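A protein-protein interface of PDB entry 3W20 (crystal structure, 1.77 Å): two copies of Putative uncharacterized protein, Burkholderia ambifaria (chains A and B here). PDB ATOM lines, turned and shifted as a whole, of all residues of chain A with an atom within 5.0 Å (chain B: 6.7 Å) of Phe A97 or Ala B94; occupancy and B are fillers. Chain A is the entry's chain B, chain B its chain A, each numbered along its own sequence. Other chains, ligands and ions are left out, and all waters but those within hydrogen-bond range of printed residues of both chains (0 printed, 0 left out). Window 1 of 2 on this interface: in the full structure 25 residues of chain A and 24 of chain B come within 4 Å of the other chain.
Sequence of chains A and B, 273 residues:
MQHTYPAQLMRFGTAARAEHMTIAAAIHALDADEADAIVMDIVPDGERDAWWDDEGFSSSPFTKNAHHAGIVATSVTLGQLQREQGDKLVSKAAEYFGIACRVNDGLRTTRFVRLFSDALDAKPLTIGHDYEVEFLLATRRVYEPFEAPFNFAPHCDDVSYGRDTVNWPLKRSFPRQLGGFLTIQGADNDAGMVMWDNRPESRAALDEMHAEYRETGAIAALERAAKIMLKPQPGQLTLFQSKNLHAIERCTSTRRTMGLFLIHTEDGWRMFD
SG of Cys B101 forms a disulfide with SG of Cys A101.
The side-chain sulfur (SG) of Cys A101 lies close to the backbone carbonyl oxygen (O) of Gly B98 (3.4 Å).
O of Ile A127 lies within hydrogen-bond range of N of Val A133, at 2.9 Å.
Among the printed residues, merely in contact across the chains: Ala A94 with Phe B97, Ala A94 with Val B133, Glu A95 with Val B133, Phe A97 with Ala B94, Gly A98 with Val B133, Ile A99 with Val B133, Ile A127 with Ser B91, Ile A127 with Ala B94, Val A133 with Ala B94, Val A133 with Glu B95, Val A133 with Gly B98 and Val A133 with Ile B99.
Of the printed residues of chain B, Ala A94 touches Phe B97 (3.3 Å) and Val B133 (3.5 Å).
Of the printed residues of chain B, Phe A97 touches Ala B94.
Printed residues of chain B within 4 Å of Cys A101: Gly B98 (3.4 Å) and Cys B101 (2.1 Å).
Of chain A, only Phe A97, Ile A127 and Val A133 come within 4 Å of Ala B94.
Printed residues of chain A within 4 Å of Phe B97: Ala A94.
The nearest printed residue of chain A that does not touch Ala B94 is Ala A93 (5.1 Å).
The nearest printed residue of chain A that does not touch Gly B98 is Phe A97 (4.2 Å).
Of the 14 printed residues of chain A, 8 touch a printed residue of chain B.
Hydrophobic or aromatic side chains of chain A within 4 Å of the printed part of chain B: Ala A94, Phe A97, Ile A127 and Val A133.
Of the 14 printed residues of chain B, 8 touch a printed residue of chain A.
Ala A94 touches Phe B97, and with the chains exchanged Phe A97 touches Ala B94.
Glu A95 touches Val B133, and with the chains exchanged Val A133 touches Glu B95.
Gly A98 touches Val B133, and with the chains exchanged Val A133 touches Gly B98.
Ile A99 touches Val B133, and with the chains exchanged Val A133 touches Ile B99.
10 positions are printed for both chains.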
ATOM      1  N   LEU A  81      13.555   4.997 -33.660  1.00  0.00           N
ATOM      2  CA  LEU A  81      14.643   4.048 -33.743  1.00  0.00           C
ATOM      3  C   LEU A  81      14.175   2.728 -34.327  1.00  0.00           C
ATOM      4  O   LEU A  81      14.837   2.094 -35.173  1.00  0.00           O
ATOM      5  CB  LEU A  81      15.272   3.884 -32.360  1.00  0.00           C
ATOM      6  CG  LEU A  81      16.437   2.960 -32.347  1.00  0.00           C
ATOM      7  CD1 LEU A  81      17.614   3.580 -33.158  1.00  0.00           C
ATOM      8  CD2 LEU A  81      16.866   2.716 -30.874  1.00  0.00           C
ATOM      9  N   ALA A  93      20.908   4.206 -33.238  1.00  0.00           N
ATOM     10  CA  ALA A  93      20.940   3.750 -31.826  1.00  0.00           C
ATOM     11  C   ALA A  93      22.035   4.530 -31.078  1.00  0.00           C
ATOM     12  O   ALA A  93      21.855   4.958 -29.923  1.00  0.00           O
ATOM     13  CB  ALA A  93      21.175   2.249 -31.691  1.00  0.00           C
ATOM     14  N   ALA A  94      23.212   4.657 -31.711  1.00  0.00           N
ATOM     15  CA  ALA A  94      24.290   5.455 -31.105  1.00  0.00           C
ATOM     16  C   ALA A  94      23.772   6.836 -30.722  1.00  0.00           C
ATOM     17  O   ALA A  94      24.034   7.304 -29.568  1.00  0.00           O
ATOM     18  CB  ALA A  94      25.473   5.605 -32.092  1.00  0.00           C
ATOM     19  N   GLU A  95      23.046   7.492 -31.627  1.00  0.00           N
ATOM     20  CA  GLU A  95      22.452   8.824 -31.343  1.00  0.00           C
ATOM     21  C   GLU A  95      21.465   8.760 -30.164  1.00  0.00           C
ATOM     22  O   GLU A  95      21.510   9.635 -29.247  1.00  0.00           O
ATOM     23  CB  GLU A  95      21.746   9.437 -32.558  1.00  0.00           C
ATOM     24  CG  GLU A  95      22.684   9.633 -33.753  1.00  0.00           C
ATOM     25  CD  GLU A  95      22.002  10.296 -34.926  1.00  0.00           C
ATOM     26  OE1 GLU A  95      21.016   9.725 -35.477  1.00  0.00           O
ATOM     27  OE2 GLU A  95      22.480  11.357 -35.301  1.00  0.00           O
ATOM     28  N   TYR A  96      20.609   7.736 -30.168  1.00  0.00           N
ATOM     29  CA  TYR A  96      19.520   7.671 -29.171  1.00  0.00           C
ATOM     30  C   TYR A  96      20.097   7.525 -27.767  1.00  0.00           C
ATOM     31  O   TYR A  96      19.748   8.287 -26.818  1.00  0.00           O
ATOM     32  CB  TYR A  96      18.540   6.569 -29.554  1.00  0.00           C
ATOM     33  CG  TYR A  96      17.487   6.295 -28.483  1.00  0.00           C
ATOM     34  CD1 TYR A  96      16.273   6.969 -28.512  1.00  0.00           C
ATOM     35  CD2 TYR A  96      17.675   5.260 -27.519  1.00  0.00           C
ATOM     36  CE1 TYR A  96      15.265   6.688 -27.568  1.00  0.00           C
ATOM     37  CE2 TYR A  96      16.679   5.010 -26.551  1.00  0.00           C
ATOM     38  CZ  TYR A  96      15.483   5.708 -26.606  1.00  0.00           C
ATOM     39  OH  TYR A  96      14.544   5.460 -25.614  1.00  0.00           O
ATOM     40  N   PHE A  97      20.998   6.543 -27.600  1.00  0.00           N
ATOM     41  CA  PHE A  97      21.591   6.298 -26.300  1.00  0.00           C
ATOM     42  C   PHE A  97      22.544   7.349 -25.866  1.00  0.00           C
ATOM     43  O   PHE A  97      22.617   7.711 -24.688  1.00  0.00           O
ATOM     44  CB  PHE A  97      22.203   4.875 -26.254  1.00  0.00           C
ATOM     45  CG  PHE A  97      21.144   3.813 -26.297  1.00  0.00           C
ATOM     46  CD1 PHE A  97      20.397   3.500 -25.143  1.00  0.00           C
ATOM     47  CD2 PHE A  97      20.831   3.186 -27.501  1.00  0.00           C
ATOM     48  CE1 PHE A  97      19.384   2.566 -25.159  1.00  0.00           C
ATOM     49  CE2 PHE A  97      19.816   2.227 -27.500  1.00  0.00           C
ATOM     50  CZ  PHE A  97      19.108   1.909 -26.347  1.00  0.00           C
ATOM     51  N   GLY A  98      23.241   7.907 -26.842  1.00  0.00           N
ATOM     52  CA  GLY A  98      24.070   9.088 -26.534  1.00  0.00           C
ATOM     53  C   GLY A  98      23.323  10.305 -26.030  1.00  0.00           C
ATOM     54  O   GLY A  98      23.745  10.925 -25.027  1.00  0.00           O
ATOM     55  N   ILE A  99      22.201  10.612 -26.657  1.00  0.00           N
ATOM     56  CA  ILE A  99      21.297  11.683 -26.174  1.00  0.00           C
ATOM     57  C   ILE A  99      20.707  11.341 -24.820  1.00  0.00           C
ATOM     58  O   ILE A  99      20.678  12.195 -23.909  1.00  0.00           O
ATOM     59  CB  ILE A  99      20.216  11.979 -27.189  1.00  0.00           C
ATOM     60  CG1 ILE A  99      20.911  12.638 -28.397  1.00  0.00           C
ATOM     61  CG2 ILE A  99      19.185  12.960 -26.655  1.00  0.00           C
ATOM     62  CD1 ILE A  99      20.018  12.752 -29.582  1.00  0.00           C
ATOM     63  N   ALA A 100      20.287  10.079 -24.619  1.00  0.00           N
ATOM     64  CA  ALA A 100      19.664   9.754 -23.317  1.00  0.00           C
ATOM     65  C   ALA A 100      20.643   9.982 -22.136  1.00  0.00           C
ATOM     66  O   ALA A 100      20.264  10.509 -21.071  1.00  0.00           O
ATOM     67  CB  ALA A 100      19.147   8.345 -23.316  1.00  0.00           C
ATOM     68  N   CYS A 101      21.883   9.613 -22.367  1.00  0.00           N
ATOM     69  CA  CYS A 101      22.967   9.838 -21.420  1.00  0.00           C
ATOM     70  C   CYS A 101      23.048  11.360 -21.116  1.00  0.00           C
ATOM     71  O   CYS A 101      23.226  11.746 -19.950  1.00  0.00           O
ATOM     72  CB  CYS A 101      24.241   9.304 -22.048  1.00  0.00           C
ATOM     73  SG  CYS A 101      25.704   9.630 -21.000  1.00  0.00           S
ATOM     74  N   ILE A 127      19.659  -1.134 -21.043  1.00  0.00           N
ATOM     75  CA  ILE A 127      20.075  -2.238 -21.909  1.00  0.00           C
ATOM     76  C   ILE A 127      21.572  -2.419 -21.641  1.00  0.00           C
ATOM     77  O   ILE A 127      22.267  -1.436 -21.275  1.00  0.00           O
ATOM     78  CB  ILE A 127      19.783  -1.895 -23.408  1.00  0.00           C
ATOM     79  CG1 ILE A 127      20.025  -3.150 -24.314  1.00  0.00           C
ATOM     80  CG2 ILE A 127      20.534  -0.602 -23.786  1.00  0.00           C
ATOM     81  CD1 ILE A 127      19.707  -2.964 -25.776  1.00  0.00           C
ATOM     82  N   VAL A 133      23.067   0.900 -19.700  1.00  0.00           N
ATOM     83  CA  VAL A 133      22.895   2.308 -20.118  1.00  0.00           C
ATOM     84  C   VAL A 133      21.412   2.590 -20.246  1.00  0.00           C
ATOM     85  O   VAL A 133      20.631   1.694 -20.509  1.00  0.00           O
ATOM     86  CB  VAL A 133      23.627   2.686 -21.470  1.00  0.00           C
ATOM     87  CG1 VAL A 133      25.160   2.510 -21.269  1.00  0.00           C
ATOM     88  CG2 VAL A 133      23.162   1.917 -22.698  1.00  0.00           C
ATOM     89  N   GLU A 134      21.056   3.851 -20.123  1.00  0.00           N
ATOM     90  CA  GLU A 134      19.579   4.178 -20.075  1.00  0.00           C
ATOM     91  C   GLU A 134      18.980   4.480 -21.447  1.00  0.00           C
ATOM     92  O   GLU A 134      19.610   5.117 -22.283  1.00  0.00           O
ATOM     93  CB  GLU A 134      19.365   5.379 -19.140  1.00  0.00           C
ATOM     94  CG  GLU A 134      19.781   5.050 -17.677  1.00  0.00           C
ATOM     95  CD  GLU A 134      19.720   6.211 -16.741  1.00  0.00           C
ATOM     96  OE1 GLU A 134      19.545   7.331 -17.211  1.00  0.00           O
ATOM     97  OE2 GLU A 134      19.864   5.955 -15.480  1.00  0.00           O
ATOM     98  N   PHE A 135      17.729   4.022 -21.658  1.00  0.00           N
ATOM     99  CA  PHE A 135      16.900   4.582 -22.688  1.00  0.00           C
ATOM    100  C   PHE A 135      16.466   5.995 -22.303  1.00  0.00           C
ATOM    101  O   PHE A 135      16.552   6.419 -21.140  1.00  0.00           O
ATOM    102  CB  PHE A 135      15.603   3.732 -22.762  1.00  0.00           C
ATOM    103  CG  PHE A 135      15.797   2.405 -23.449  1.00  0.00           C
ATOM    104  CD1 PHE A 135      15.279   2.207 -24.711  1.00  0.00           C
ATOM    105  CD2 PHE A 135      16.482   1.353 -22.829  1.00  0.00           C
ATOM    106  CE1 PHE A 135      15.445   0.966 -25.336  1.00  0.00           C
ATOM    107  CE2 PHE A 135      16.695   0.122 -23.458  1.00  0.00           C
ATOM    108  CZ  PHE A 135      16.178  -0.068 -24.725  1.00  0.00           C
ATOM    109  N   LEU B  81      33.678  -3.186 -29.986  1.00  0.00           N
ATOM    110  CA  LEU B  81      32.394  -2.986 -30.635  1.00  0.00           C
ATOM    111  C   LEU B  81      32.391  -3.582 -32.033  1.00  0.00           C
ATOM    112  O   LEU B  81      31.383  -4.126 -32.473  1.00  0.00           O
ATOM    113  CB  LEU B  81      32.015  -1.500 -30.638  1.00  0.00           C
ATOM    114  CG  LEU B  81      30.700  -1.063 -31.325  1.00  0.00           C
ATOM    115  CD1 LEU B  81      29.497  -1.775 -30.698  1.00  0.00           C
ATOM    116  CD2 LEU B  81      30.537   0.434 -31.261  1.00  0.00           C
ATOM    117  N   LEU B  89      25.414  -6.173 -32.109  1.00  0.00           N
ATOM    118  CA  LEU B  89      26.110  -4.943 -32.450  1.00  0.00           C
ATOM    119  C   LEU B  89      25.218  -3.751 -32.064  1.00  0.00           C
ATOM    120  O   LEU B  89      25.714  -2.760 -31.519  1.00  0.00           O
ATOM    121  CB  LEU B  89      26.414  -4.888 -33.943  1.00  0.00           C
ATOM    122  CG  LEU B  89      26.790  -3.582 -34.499  1.00  0.00           C
ATOM    123  CD1 LEU B  89      28.151  -3.215 -33.876  1.00  0.00           C
ATOM    124  CD2 LEU B  89      27.017  -3.709 -36.014  1.00  0.00           C
ATOM    125  N   VAL B  90      23.893  -3.861 -32.293  1.00  0.00           N
ATOM    126  CA  VAL B  90      22.993  -2.721 -31.853  1.00  0.00           C
ATOM    127  C   VAL B  90      23.080  -2.531 -30.319  1.00  0.00           C
ATOM    128  O   VAL B  90      23.259  -1.385 -29.835  1.00  0.00           O
ATOM    129  CB  VAL B  90      21.556  -2.974 -32.285  1.00  0.00           C
ATOM    130  CG1 VAL B  90      20.652  -1.854 -31.802  1.00  0.00           C
ATOM    131  CG2 VAL B  90      21.433  -3.042 -33.851  1.00  0.00           C
ATOM    132  N   SER B  91      23.062  -3.639 -29.571  1.00  0.00           N
ATOM    133  CA  SER B  91      23.036  -3.543 -28.108  1.00  0.00           C
ATOM    134  C   SER B  91      24.405  -3.092 -27.607  1.00  0.00           C
ATOM    135  O   SER B  91      24.492  -2.253 -26.715  1.00  0.00           O
ATOM    136  CB  SER B  91      22.591  -4.832 -27.384  1.00  0.00           C
ATOM    137  OG  SER B  91      23.412  -5.878 -27.777  1.00  0.00           O
ATOM    138  N   LYS B  92      25.495  -3.621 -28.176  1.00  0.00           N
ATOM    139  CA  LYS B  92      26.846  -3.123 -27.742  1.00  0.00           C
ATOM    140  C   LYS B  92      27.077  -1.685 -28.143  1.00  0.00           C
ATOM    141  O   LYS B  92      27.778  -0.981 -27.399  1.00  0.00           O
ATOM    142  CB  LYS B  92      27.980  -4.005 -28.261  1.00  0.00           C
ATOM    143  CG  LYS B  92      29.284  -3.902 -27.496  1.00  0.00           C
ATOM    144  CD  LYS B  92      29.070  -4.370 -26.062  1.00  0.00           C
ATOM    145  CE  LYS B  92      30.313  -4.872 -25.335  1.00  0.00           C
ATOM    146  NZ  LYS B  92      30.570  -6.324 -25.555  1.00  0.00           N
ATOM    147  N   ALA B  93      26.527  -1.237 -29.302  1.00  0.00           N
ATOM    148  CA  ALA B  93      26.654   0.219 -29.681  1.00  0.00           C
ATOM    149  C   ALA B  93      25.942   1.055 -28.628  1.00  0.00           C
ATOM    150  O   ALA B  93      26.421   2.129 -28.273  1.00  0.00           O
ATOM    151  CB  ALA B  93      26.049   0.507 -31.082  1.00  0.00           C
ATOM    152  N   ALA B  94      24.785   0.582 -28.131  1.00  0.00           N
ATOM    153  CA  ALA B  94      24.086   1.387 -27.119  1.00  0.00           C
ATOM    154  C   ALA B  94      25.029   1.499 -25.900  1.00  0.00           C
ATOM    155  O   ALA B  94      25.110   2.581 -25.322  1.00  0.00           O
ATOM    156  CB  ALA B  94      22.800   0.659 -26.639  1.00  0.00           C
ATOM    157  N   GLU B  95      25.662   0.404 -25.470  1.00  0.00           N
ATOM    158  CA  GLU B  95      26.617   0.445 -24.321  1.00  0.00           C
ATOM    159  C   GLU B  95      27.785   1.356 -24.594  1.00  0.00           C
ATOM    160  O   GLU B  95      28.135   2.258 -23.783  1.00  0.00           O
ATOM    161  CB  GLU B  95      27.178  -0.956 -23.907  1.00  0.00           C
ATOM    162  CG  GLU B  95      26.187  -1.913 -23.286  1.00  0.00           C
ATOM    163  CD  GLU B  95      26.948  -3.223 -22.989  1.00  0.00           C
ATOM    164  OE1 GLU B  95      27.945  -3.199 -22.209  1.00  0.00           O
ATOM    165  OE2 GLU B  95      26.605  -4.226 -23.608  1.00  0.00           O
ATOM    166  N   TYR B  96      28.330   1.226 -25.792  1.00  0.00           N
ATOM    167  CA  TYR B  96      29.504   2.016 -26.136  1.00  0.00           C
ATOM    168  C   TYR B  96      29.215   3.504 -26.085  1.00  0.00           C
ATOM    169  O   TYR B  96      29.956   4.267 -25.402  1.00  0.00           O
ATOM    170  CB  TYR B  96      30.017   1.623 -27.515  1.00  0.00           C
ATOM    171  CG  TYR B  96      31.257   2.416 -27.922  1.00  0.00           C
ATOM    172  CD1 TYR B  96      32.543   2.057 -27.515  1.00  0.00           C
ATOM    173  CD2 TYR B  96      31.121   3.522 -28.753  1.00  0.00           C
ATOM    174  CE1 TYR B  96      33.659   2.825 -27.941  1.00  0.00           C
ATOM    175  CE2 TYR B  96      32.218   4.277 -29.180  1.00  0.00           C
ATOM    176  CZ  TYR B  96      33.471   3.927 -28.761  1.00  0.00           C
ATOM    177  OH  TYR B  96      34.541   4.684 -29.181  1.00  0.00           O
ATOM    178  N   PHE B  97      28.171   3.915 -26.757  1.00  0.00           N
ATOM    179  CA  PHE B  97      27.876   5.366 -26.838  1.00  0.00           C
ATOM    180  C   PHE B  97      27.268   5.902 -25.569  1.00  0.00           C
ATOM    181  O   PHE B  97      27.539   7.046 -25.225  1.00  0.00           O
ATOM    182  CB  PHE B  97      27.033   5.674 -28.075  1.00  0.00           C
ATOM    183  CG  PHE B  97      27.879   5.574 -29.310  1.00  0.00           C
ATOM    184  CD1 PHE B  97      28.802   6.573 -29.632  1.00  0.00           C
ATOM    185  CD2 PHE B  97      27.783   4.432 -30.103  1.00  0.00           C
ATOM    186  CE1 PHE B  97      29.619   6.426 -30.767  1.00  0.00           C
ATOM    187  CE2 PHE B  97      28.602   4.261 -31.218  1.00  0.00           C
ATOM    188  CZ  PHE B  97      29.490   5.294 -31.544  1.00  0.00           C
ATOM    189  N   GLY B  98      26.565   5.052 -24.847  1.00  0.00           N
ATOM    190  CA  GLY B  98      25.960   5.455 -23.539  1.00  0.00           C
ATOM    191  C   GLY B  98      27.085   5.685 -22.531  1.00  0.00           C
ATOM    192  O   GLY B  98      27.090   6.658 -21.740  1.00  0.00           O
ATOM    193  N   ILE B  99      28.088   4.846 -22.574  1.00  0.00           N
ATOM    194  CA  ILE B  99      29.223   4.969 -21.625  1.00  0.00           C
ATOM    195  C   ILE B  99      30.070   6.181 -21.968  1.00  0.00           C
ATOM    196  O   ILE B  99      30.483   6.928 -21.082  1.00  0.00           O
ATOM    197  CB  ILE B  99      30.099   3.707 -21.602  1.00  0.00           C
ATOM    198  CG1 ILE B  99      29.339   2.590 -20.872  1.00  0.00           C
ATOM    199  CG2 ILE B  99      31.415   3.891 -20.842  1.00  0.00           C
ATOM    200  CD1 ILE B  99      30.032   1.260 -21.033  1.00  0.00           C
ATOM    201  N   CYS B 101      29.561   8.995 -23.097  1.00  0.00           N
ATOM    202  CA  CYS B 101      29.075  10.220 -22.602  1.00  0.00           C
ATOM    203  C   CYS B 101      29.303  10.389 -21.076  1.00  0.00           C
ATOM    204  O   CYS B 101      29.618  11.486 -20.665  1.00  0.00           O
ATOM    205  CB  CYS B 101      27.666  10.458 -23.133  1.00  0.00           C
ATOM    206  SG  CYS B 101      26.550  11.264 -21.957  1.00  0.00           S
ATOM    207  N   VAL B 133      26.908  12.734 -31.041  1.00  0.00           N
ATOM    208  CA  VAL B 133      27.250  12.120 -29.769  1.00  0.00           C
ATOM    209  C   VAL B 133      28.696  11.605 -29.990  1.00  0.00           C
ATOM    210  O   VAL B 133      29.118  11.375 -31.116  1.00  0.00           O
ATOM    211  CB  VAL B 133      26.255  11.023 -29.378  1.00  0.00           C
ATOM    212  CG1 VAL B 133      24.796  11.538 -29.497  1.00  0.00           C
ATOM    213  CG2 VAL B 133      26.486   9.751 -30.136  1.00  0.00           C
